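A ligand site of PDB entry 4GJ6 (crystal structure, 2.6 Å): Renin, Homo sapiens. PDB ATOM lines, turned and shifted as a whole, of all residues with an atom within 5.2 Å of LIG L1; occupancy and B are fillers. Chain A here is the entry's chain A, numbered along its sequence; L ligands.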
ATOM      1  N   VAL A  36     -29.460 -30.368  14.996  1.00  0.00           N
ATOM      2  CA  VAL A  36     -28.429 -30.573  14.012  1.00  0.00           C
ATOM      3  C   VAL A  36     -28.232 -32.111  13.997  1.00  0.00           C
ATOM      4  O   VAL A  36     -28.133 -32.744  15.066  1.00  0.00           O
ATOM      5  CB  VAL A  36     -27.121 -29.838  14.396  1.00  0.00           C
ATOM      6  CG1 VAL A  36     -25.917 -30.454  13.690  1.00  0.00           C
ATOM      7  CG2 VAL A  36     -27.216 -28.339  14.128  1.00  0.00           C
ATOM      8  N   ASP A  38     -25.752 -34.770  13.245  1.00  0.00           N
ATOM      9  CA  ASP A  38     -24.305 -34.802  13.309  1.00  0.00           C
ATOM     10  C   ASP A  38     -23.662 -36.163  13.186  1.00  0.00           C
ATOM     11  O   ASP A  38     -23.697 -36.938  14.140  1.00  0.00           O
ATOM     12  CB  ASP A  38     -23.910 -34.117  14.638  1.00  0.00           C
ATOM     13  CG  ASP A  38     -22.441 -33.976  14.950  1.00  0.00           C
ATOM     14  OD1 ASP A  38     -21.629 -33.999  14.002  1.00  0.00           O
ATOM     15  OD2 ASP A  38     -22.108 -33.759  16.136  1.00  0.00           O
ATOM     16  N   GLY A  40     -20.504 -36.598  13.223  1.00  0.00           N
ATOM     17  CA  GLY A  40     -19.327 -36.501  14.069  1.00  0.00           C
ATOM     18  C   GLY A  40     -19.559 -36.927  15.510  1.00  0.00           C
ATOM     19  O   GLY A  40     -18.597 -37.069  16.247  1.00  0.00           O
ATOM     20  N   SER A  41     -20.815 -37.101  15.951  1.00  0.00           N
ATOM     21  CA  SER A  41     -21.139 -37.544  17.313  1.00  0.00           C
ATOM     22  C   SER A  41     -22.214 -38.654  17.339  1.00  0.00           C
ATOM     23  O   SER A  41     -22.874 -38.891  16.306  1.00  0.00           O
ATOM     24  CB  SER A  41     -21.442 -36.380  18.235  1.00  0.00           C
ATOM     25  OG  SER A  41     -22.676 -35.737  17.953  1.00  0.00           O
ATOM     26  N   TYR A  83     -17.198 -30.702  24.532  1.00  0.00           N
ATOM     27  CA  TYR A  83     -17.127 -29.862  23.337  1.00  0.00           C
ATOM     28  C   TYR A  83     -15.793 -29.067  23.401  1.00  0.00           C
ATOM     29  O   TYR A  83     -15.143 -29.071  24.451  1.00  0.00           O
ATOM     30  CB  TYR A  83     -18.370 -28.972  23.212  1.00  0.00           C
ATOM     31  CG  TYR A  83     -19.547 -29.712  22.610  1.00  0.00           C
ATOM     32  CD1 TYR A  83     -20.417 -30.448  23.403  1.00  0.00           C
ATOM     33  CD2 TYR A  83     -19.766 -29.713  21.234  1.00  0.00           C
ATOM     34  CE1 TYR A  83     -21.491 -31.157  22.837  1.00  0.00           C
ATOM     35  CE2 TYR A  83     -20.818 -30.425  20.665  1.00  0.00           C
ATOM     36  CZ  TYR A  83     -21.685 -31.137  21.466  1.00  0.00           C
ATOM     37  OH  TYR A  83     -22.735 -31.825  20.905  1.00  0.00           O
ATOM     38  N   PRO A 118     -20.510 -22.435  22.062  1.00  0.00           N
ATOM     39  CA  PRO A 118     -21.184 -21.709  20.957  1.00  0.00           C
ATOM     40  C   PRO A 118     -22.690 -21.503  21.102  1.00  0.00           C
ATOM     41  O   PRO A 118     -23.281 -20.793  20.291  1.00  0.00           O
ATOM     42  CB  PRO A 118     -20.942 -22.632  19.766  1.00  0.00           C
ATOM     43  CG  PRO A 118     -20.964 -24.012  20.364  1.00  0.00           C
ATOM     44  CD  PRO A 118     -20.384 -23.876  21.757  1.00  0.00           C
ATOM     45  N   PHE A 119     -23.316 -22.116  22.109  1.00  0.00           N
ATOM     46  CA  PHE A 119     -24.775 -22.170  22.306  1.00  0.00           C
ATOM     47  C   PHE A 119     -25.595 -20.894  22.264  1.00  0.00           C
ATOM     48  O   PHE A 119     -26.732 -20.948  21.794  1.00  0.00           O
ATOM     49  CB  PHE A 119     -25.181 -23.156  23.421  1.00  0.00           C
ATOM     50  CG  PHE A 119     -24.559 -24.506  23.108  1.00  0.00           C
ATOM     51  CD1 PHE A 119     -25.021 -25.279  22.045  1.00  0.00           C
ATOM     52  CD2 PHE A 119     -23.414 -24.942  23.781  1.00  0.00           C
ATOM     53  CE1 PHE A 119     -24.398 -26.479  21.702  1.00  0.00           C
ATOM     54  CE2 PHE A 119     -22.783 -26.138  23.437  1.00  0.00           C
ATOM     55  CZ  PHE A 119     -23.277 -26.901  22.398  1.00  0.00           C
ATOM     56  N   PHE A 124     -30.502 -23.574  16.610  1.00  0.00           N
ATOM     57  CA  PHE A 124     -31.063 -24.894  16.898  1.00  0.00           C
ATOM     58  C   PHE A 124     -31.048 -25.177  18.399  1.00  0.00           C
ATOM     59  O   PHE A 124     -30.281 -24.557  19.141  1.00  0.00           O
ATOM     60  CB  PHE A 124     -30.290 -25.986  16.105  1.00  0.00           C
ATOM     61  CG  PHE A 124     -28.826 -26.040  16.441  1.00  0.00           C
ATOM     62  CD1 PHE A 124     -27.908 -25.252  15.749  1.00  0.00           C
ATOM     63  CD2 PHE A 124     -28.360 -26.851  17.456  1.00  0.00           C
ATOM     64  CE1 PHE A 124     -26.561 -25.255  16.096  1.00  0.00           C
ATOM     65  CE2 PHE A 124     -27.012 -26.854  17.812  1.00  0.00           C
ATOM     66  CZ  PHE A 124     -26.129 -26.057  17.124  1.00  0.00           C
ATOM     67  N   VAL A 127     -28.841 -31.699  19.540  1.00  0.00           N
ATOM     68  CA  VAL A 127     -28.038 -32.479  18.622  1.00  0.00           C
ATOM     69  C   VAL A 127     -28.555 -33.916  18.529  1.00  0.00           C
ATOM     70  O   VAL A 127     -28.941 -34.476  19.533  1.00  0.00           O
ATOM     71  CB  VAL A 127     -26.541 -32.411  19.067  1.00  0.00           C
ATOM     72  CG1 VAL A 127     -25.675 -33.401  18.296  1.00  0.00           C
ATOM     73  CG2 VAL A 127     -25.982 -30.992  18.955  1.00  0.00           C
ATOM     74  N   GLN A 135     -18.585 -44.597  19.698  1.00  0.00           N
ATOM     75  CA  GLN A 135     -18.309 -43.251  20.181  1.00  0.00           C
ATOM     76  C   GLN A 135     -19.479 -42.597  21.002  1.00  0.00           C
ATOM     77  O   GLN A 135     -19.405 -41.420  21.360  1.00  0.00           O
ATOM     78  CB  GLN A 135     -17.882 -42.364  19.019  1.00  0.00           C
ATOM     79  CG  GLN A 135     -16.485 -42.664  18.481  1.00  0.00           C
ATOM     80  CD  GLN A 135     -16.211 -41.698  17.373  1.00  0.00           C
ATOM     81  OE1 GLN A 135     -16.688 -41.885  16.243  1.00  0.00           O
ATOM     82  NE2 GLN A 135     -15.549 -40.598  17.683  1.00  0.00           N
ATOM     83  N   LEU A 224     -12.519 -36.906   8.417  1.00  0.00           N
ATOM     84  CA  LEU A 224     -13.776 -37.185   9.077  1.00  0.00           C
ATOM     85  C   LEU A 224     -14.890 -36.491   8.282  1.00  0.00           C
ATOM     86  O   LEU A 224     -14.794 -35.293   7.980  1.00  0.00           O
ATOM     87  CB  LEU A 224     -13.694 -36.677  10.528  1.00  0.00           C
ATOM     88  CG  LEU A 224     -14.920 -36.896  11.403  1.00  0.00           C
ATOM     89  CD1 LEU A 224     -15.012 -38.338  11.883  1.00  0.00           C
ATOM     90  CD2 LEU A 224     -14.896 -35.931  12.599  1.00  0.00           C
ATOM     91  N   ASP A 226     -18.011 -35.011   8.657  1.00  0.00           N
ATOM     92  CA  ASP A 226     -18.791 -34.445   9.737  1.00  0.00           C
ATOM     93  C   ASP A 226     -19.827 -33.445   9.266  1.00  0.00           C
ATOM     94  O   ASP A 226     -19.501 -32.306   8.959  1.00  0.00           O
ATOM     95  CB  ASP A 226     -17.861 -33.797  10.770  1.00  0.00           C
ATOM     96  CG  ASP A 226     -18.456 -33.605  12.155  1.00  0.00           C
ATOM     97  OD1 ASP A 226     -19.699 -33.607  12.270  1.00  0.00           O
ATOM     98  OD2 ASP A 226     -17.676 -33.450  13.118  1.00  0.00           O
ATOM     99  N   GLY A 228     -22.035 -32.158  11.144  1.00  0.00           N
ATOM    100  CA  GLY A 228     -22.209 -31.262  12.279  1.00  0.00           C
ATOM    101  C   GLY A 228     -21.244 -30.098  12.314  1.00  0.00           C
ATOM    102  O   GLY A 228     -21.462 -29.140  13.036  1.00  0.00           O
ATOM    103  N   ALA A 229     -20.146 -30.176  11.536  1.00  0.00           N
ATOM    104  CA  ALA A 229     -19.128 -29.145  11.422  1.00  0.00           C
ATOM    105  C   ALA A 229     -19.513 -28.163  10.315  1.00  0.00           C
ATOM    106  O   ALA A 229     -19.926 -28.593   9.253  1.00  0.00           O
ATOM    107  CB  ALA A 229     -17.771 -29.790  11.143  1.00  0.00           C
ATOM    108  N   SER A 230     -19.409 -26.857  10.569  1.00  0.00           N
ATOM    109  CA  SER A 230     -19.786 -25.773   9.637  1.00  0.00           C
ATOM    110  C   SER A 230     -18.872 -25.694   8.416  1.00  0.00           C
ATOM    111  O   SER A 230     -19.319 -25.308   7.336  1.00  0.00           O
ATOM    112  CB  SER A 230     -19.740 -24.418  10.350  1.00  0.00           C
ATOM    113  OG  SER A 230     -20.660 -24.317  11.438  1.00  0.00           O
ATOM    114  N   TYR A 231     -17.577 -26.001   8.618  1.00  0.00           N
ATOM    115  CA  TYR A 231     -16.522 -25.830   7.636  1.00  0.00           C
ATOM    116  C   TYR A 231     -15.720 -27.086   7.325  1.00  0.00           C
ATOM    117  O   TYR A 231     -15.982 -28.142   7.912  1.00  0.00           O
ATOM    118  CB  TYR A 231     -15.539 -24.802   8.224  1.00  0.00           C
ATOM    119  CG  TYR A 231     -16.200 -23.582   8.792  1.00  0.00           C
ATOM    120  CD1 TYR A 231     -16.894 -22.698   7.973  1.00  0.00           C
ATOM    121  CD2 TYR A 231     -16.136 -23.309  10.150  1.00  0.00           C
ATOM    122  CE1 TYR A 231     -17.536 -21.568   8.504  1.00  0.00           C
ATOM    123  CE2 TYR A 231     -16.758 -22.171  10.688  1.00  0.00           C
ATOM    124  CZ  TYR A 231     -17.455 -21.310   9.861  1.00  0.00           C
ATOM    125  OH  TYR A 231     -18.053 -20.196  10.357  1.00  0.00           O
ATOM    126  N   MET A 303      -9.197 -26.846  13.280  1.00  0.00           N
ATOM    127  CA  MET A 303      -9.882 -27.525  14.360  1.00  0.00           C
ATOM    128  C   MET A 303      -9.009 -28.687  14.771  1.00  0.00           C
ATOM    129  O   MET A 303      -8.715 -29.573  13.944  1.00  0.00           O
ATOM    130  CB  MET A 303     -11.286 -27.954  13.937  1.00  0.00           C
ATOM    131  CG  MET A 303     -12.104 -28.588  15.051  1.00  0.00           C
ATOM    132  SD  MET A 303     -13.898 -28.602  14.731  1.00  0.00           S
ATOM    133  CE  MET A 303     -14.038 -29.809  13.424  1.00  0.00           C
ATOM    134  N   ILE A 305      -8.991 -31.693  16.450  1.00  0.00           N
ATOM    135  CA  ILE A 305      -9.816 -32.781  16.968  1.00  0.00           C
ATOM    136  C   ILE A 305      -8.937 -33.697  17.847  1.00  0.00           C
ATOM    137  O   ILE A 305      -7.848 -34.108  17.425  1.00  0.00           O
ATOM    138  CB  ILE A 305     -10.592 -33.530  15.832  1.00  0.00           C
ATOM    139  CG1 ILE A 305     -11.588 -32.561  15.176  1.00  0.00           C
ATOM    140  CG2 ILE A 305     -11.337 -34.747  16.389  1.00  0.00           C
ATOM    141  CD1 ILE A 305     -11.768 -32.751  13.777  1.00  0.00           C
ATOM    142  N   PRO A 306      -9.354 -33.942  19.118  1.00  0.00           N
ATOM    143  CA  PRO A 306      -8.527 -34.782  19.998  1.00  0.00           C
ATOM    144  C   PRO A 306      -8.592 -36.268  19.679  1.00  0.00           C
ATOM    145  O   PRO A 306      -9.630 -36.756  19.215  1.00  0.00           O
ATOM    146  CB  PRO A 306      -9.125 -34.527  21.389  1.00  0.00           C
ATOM    147  CG  PRO A 306     -10.520 -34.174  21.147  1.00  0.00           C
ATOM    148  CD  PRO A 306     -10.579 -33.496  19.817  1.00  0.00           C
ATOM    149  N   THR A 309     -10.240 -40.053  17.629  1.00  0.00           N
ATOM    150  CA  THR A 309     -10.663 -39.607  16.300  1.00  0.00           C
ATOM    151  C   THR A 309      -9.611 -38.722  15.595  1.00  0.00           C
ATOM    152  O   THR A 309      -9.381 -38.885  14.385  1.00  0.00           O
ATOM    153  CB  THR A 309     -12.092 -38.984  16.326  1.00  0.00           C
ATOM    154  OG1 THR A 309     -12.979 -39.791  17.106  1.00  0.00           O
ATOM    155  CG2 THR A 309     -12.677 -38.787  14.922  1.00  0.00           C
HETATM  156  N1  LIG L   1     -19.356 -33.004  15.197  1.00  0.00           N
HETATM  157  C1  LIG L   1     -19.530 -31.557  15.054  1.00  0.00           C
HETATM  158  C2  LIG L   1     -18.432 -30.898  15.933  1.00  0.00           C
HETATM  159  C3  LIG L   1     -17.692 -32.067  16.594  1.00  0.00           C
HETATM  160  C4  LIG L   1     -18.709 -33.209  16.483  1.00  0.00           C
HETATM  161  C5  LIG L   1     -16.284 -32.351  16.022  1.00  0.00           C
HETATM  162  C6  LIG L   1     -15.657 -33.599  16.662  1.00  0.00           C
HETATM  163  C7  LIG L   1     -18.955 -29.895  16.983  1.00  0.00           C
HETATM  164  N2  LIG L   1     -19.728 -28.770  16.421  1.00  0.00           N
HETATM  165  C8  LIG L   1     -19.176 -27.861  15.565  1.00  0.00           C
HETATM  166  C9  LIG L   1     -20.994 -28.581  16.890  1.00  0.00           C
HETATM  167  C10 LIG L   1     -17.763 -27.704  15.549  1.00  0.00           C
HETATM  168  C11 LIG L   1     -17.171 -26.703  14.773  1.00  0.00           C
HETATM  169  C12 LIG L   1     -17.988 -25.868  14.013  1.00  0.00           C
HETATM  170  C13 LIG L   1     -19.385 -25.986  14.024  1.00  0.00           C
HETATM  171  C14 LIG L   1     -19.963 -26.960  14.827  1.00  0.00           C
HETATM  172  C15 LIG L   1     -21.258 -27.743  17.999  1.00  0.00           C
HETATM  173  C16 LIG L   1     -22.566 -27.592  18.516  1.00  0.00           C
HETATM  174  C17 LIG L   1     -23.618 -28.314  17.928  1.00  0.00           C
HETATM  175  C18 LIG L   1     -23.366 -29.167  16.841  1.00  0.00           C
HETATM  176  C19 LIG L   1     -22.067 -29.290  16.333  1.00  0.00           C
HETATM  177  C20 LIG L   1     -15.734 -34.857  15.997  1.00  0.00           C
HETATM  178  C21 LIG L   1     -15.175 -36.015  16.568  1.00  0.00           C
HETATM  179  C22 LIG L   1     -14.525 -35.918  17.814  1.00  0.00           C
HETATM  180  C23 LIG L   1     -14.452 -34.671  18.490  1.00  0.00           C
HETATM  181  C24 LIG L   1     -15.007 -33.502  17.907  1.00  0.00           C
HETATM  182 CL1  LIG L   1     -17.290 -24.568  13.073  1.00  0.00          CL
HETATM  183  N1  LG2 L   2     -19.148 -19.659  12.873  1.00  0.00           N
HETATM  184  C1  LG2 L   2     -18.474 -20.516  13.844  1.00  0.00           C
HETATM  185  C2  LG2 L   2     -19.577 -21.269  14.628  1.00  0.00           C
HETATM  186  C3  LG2 L   2     -20.910 -20.921  13.923  1.00  0.00           C
HETATM  187  C4  LG2 L   2     -20.437 -20.299  12.581  1.00  0.00           C
HETATM  188  C5  LG2 L   2     -21.954 -22.054  13.734  1.00  0.00           C
HETATM  189  C6  LG2 L   2     -22.429 -22.687  15.037  1.00  0.00           C
HETATM  190  C7  LG2 L   2     -19.627 -20.954  16.138  1.00  0.00           C
HETATM  191  N2  LG2 L   2     -18.444 -21.297  16.942  1.00  0.00           N
HETATM  192  C8  LG2 L   2     -18.241 -22.588  17.395  1.00  0.00           C
HETATM  193  C9  LG2 L   2     -17.686 -20.232  17.363  1.00  0.00           C
HETATM  194  C10 LG2 L   2     -17.270 -22.819  18.389  1.00  0.00           C
HETATM  195  C11 LG2 L   2     -17.111 -24.093  18.958  1.00  0.00           C
HETATM  196  C12 LG2 L   2     -17.929 -25.160  18.575  1.00  0.00           C
HETATM  197  C13 LG2 L   2     -18.917 -24.957  17.604  1.00  0.00           C
HETATM  198  C14 LG2 L   2     -19.065 -23.689  17.025  1.00  0.00           C
HETATM  199  C15 LG2 L   2     -16.429 -19.941  16.803  1.00  0.00           C
HETATM  200  C16 LG2 L   2     -15.708 -18.805  17.234  1.00  0.00           C
HETATM  201  C17 LG2 L   2     -16.239 -17.925  18.202  1.00  0.00           C
HETATM  202  C18 LG2 L   2     -17.489 -18.224  18.782  1.00  0.00           C
HETATM  203  C19 LG2 L   2     -18.201 -19.356  18.350  1.00  0.00           C
HETATM  204  C20 LG2 L   2     -22.192 -24.056  15.148  1.00  0.00           C
HETATM  205  C21 LG2 L   2     -22.596 -24.728  16.313  1.00  0.00           C
HETATM  206  C22 LG2 L   2     -23.230 -24.072  17.369  1.00  0.00           C
HETATM  207  C23 LG2 L   2     -23.502 -22.696  17.262  1.00  0.00           C
HETATM  208  C24 LG2 L   2     -23.097 -22.001  16.096  1.00  0.00           C
HETATM  209 CL1  LG2 L   2     -17.713 -26.732  19.307  1.00  0.00          CL
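A nitrogen (N1) of LIG L1 is in salt-bridge range of the side-chain carboxylate of Asp 226, at 2.7 Å.
A nitrogen (N1) of LIG L1 lies within salt-bridge range of the side-chain carboxylate (OD1) of Asp 38 (2.8 Å).
A nitrogen (N1) of LG2 L2 lies within hydrogen-bond range of the side-chain hydroxyl (OH) of Tyr 231 (2.8 Å).
OD1 of Asp 226 lies close to OD1 of Asp 38 (2.6 Å).
The side-chain carboxylate of Asp 226 sits at hydrogen-bond distance from the backbone NH of Gly 228, at 3.0 Å.
OD1 of Asp 226 is in hydrogen-bond range of N of Gly 40 (3.2 Å).
The side-chain carboxylate of Asp 38 sits close to the backbone NH of Gly 228 (3.4 Å).
The side-chain carboxylate of Asp 38 sits at hydrogen-bond distance from the backbone NH of Gly 40 (2.9 Å).
OD2 of Asp 38 sits at hydrogen-bond distance from OG of Ser 41 (2.7 Å).
Gly 40 touches LIG L1.
Tyr 83 touches LIG L1.
Phe 119 touches LIG L1 (CE1 to C16, 3.8 Å).
Phe 124 touches LIG L1.
Val 127 touches LIG L1 (CG2 to C17, 3.7 Å).
CD2 of Leu 224 touches C20 of LIG L1, at 3.7 Å.
Gly 228 touches LIG L1 (O to C14, 3.2 Å).
N of Ala 229 touches C1 of LIG L1 (3.8 Å).
OG of Ser 230 touches C13 of LIG L1, 3.3 Å away.
Tyr 231 touches LIG L1 (CD2 to CL1, 3.4 Å).
SD of Met 303 touches C11 of LIG L1 (3.8 Å).
Ile 305 touches LIG L1.
The nearest printed residue that does not touch LIG L1 is Thr 309 (4.1 Å).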
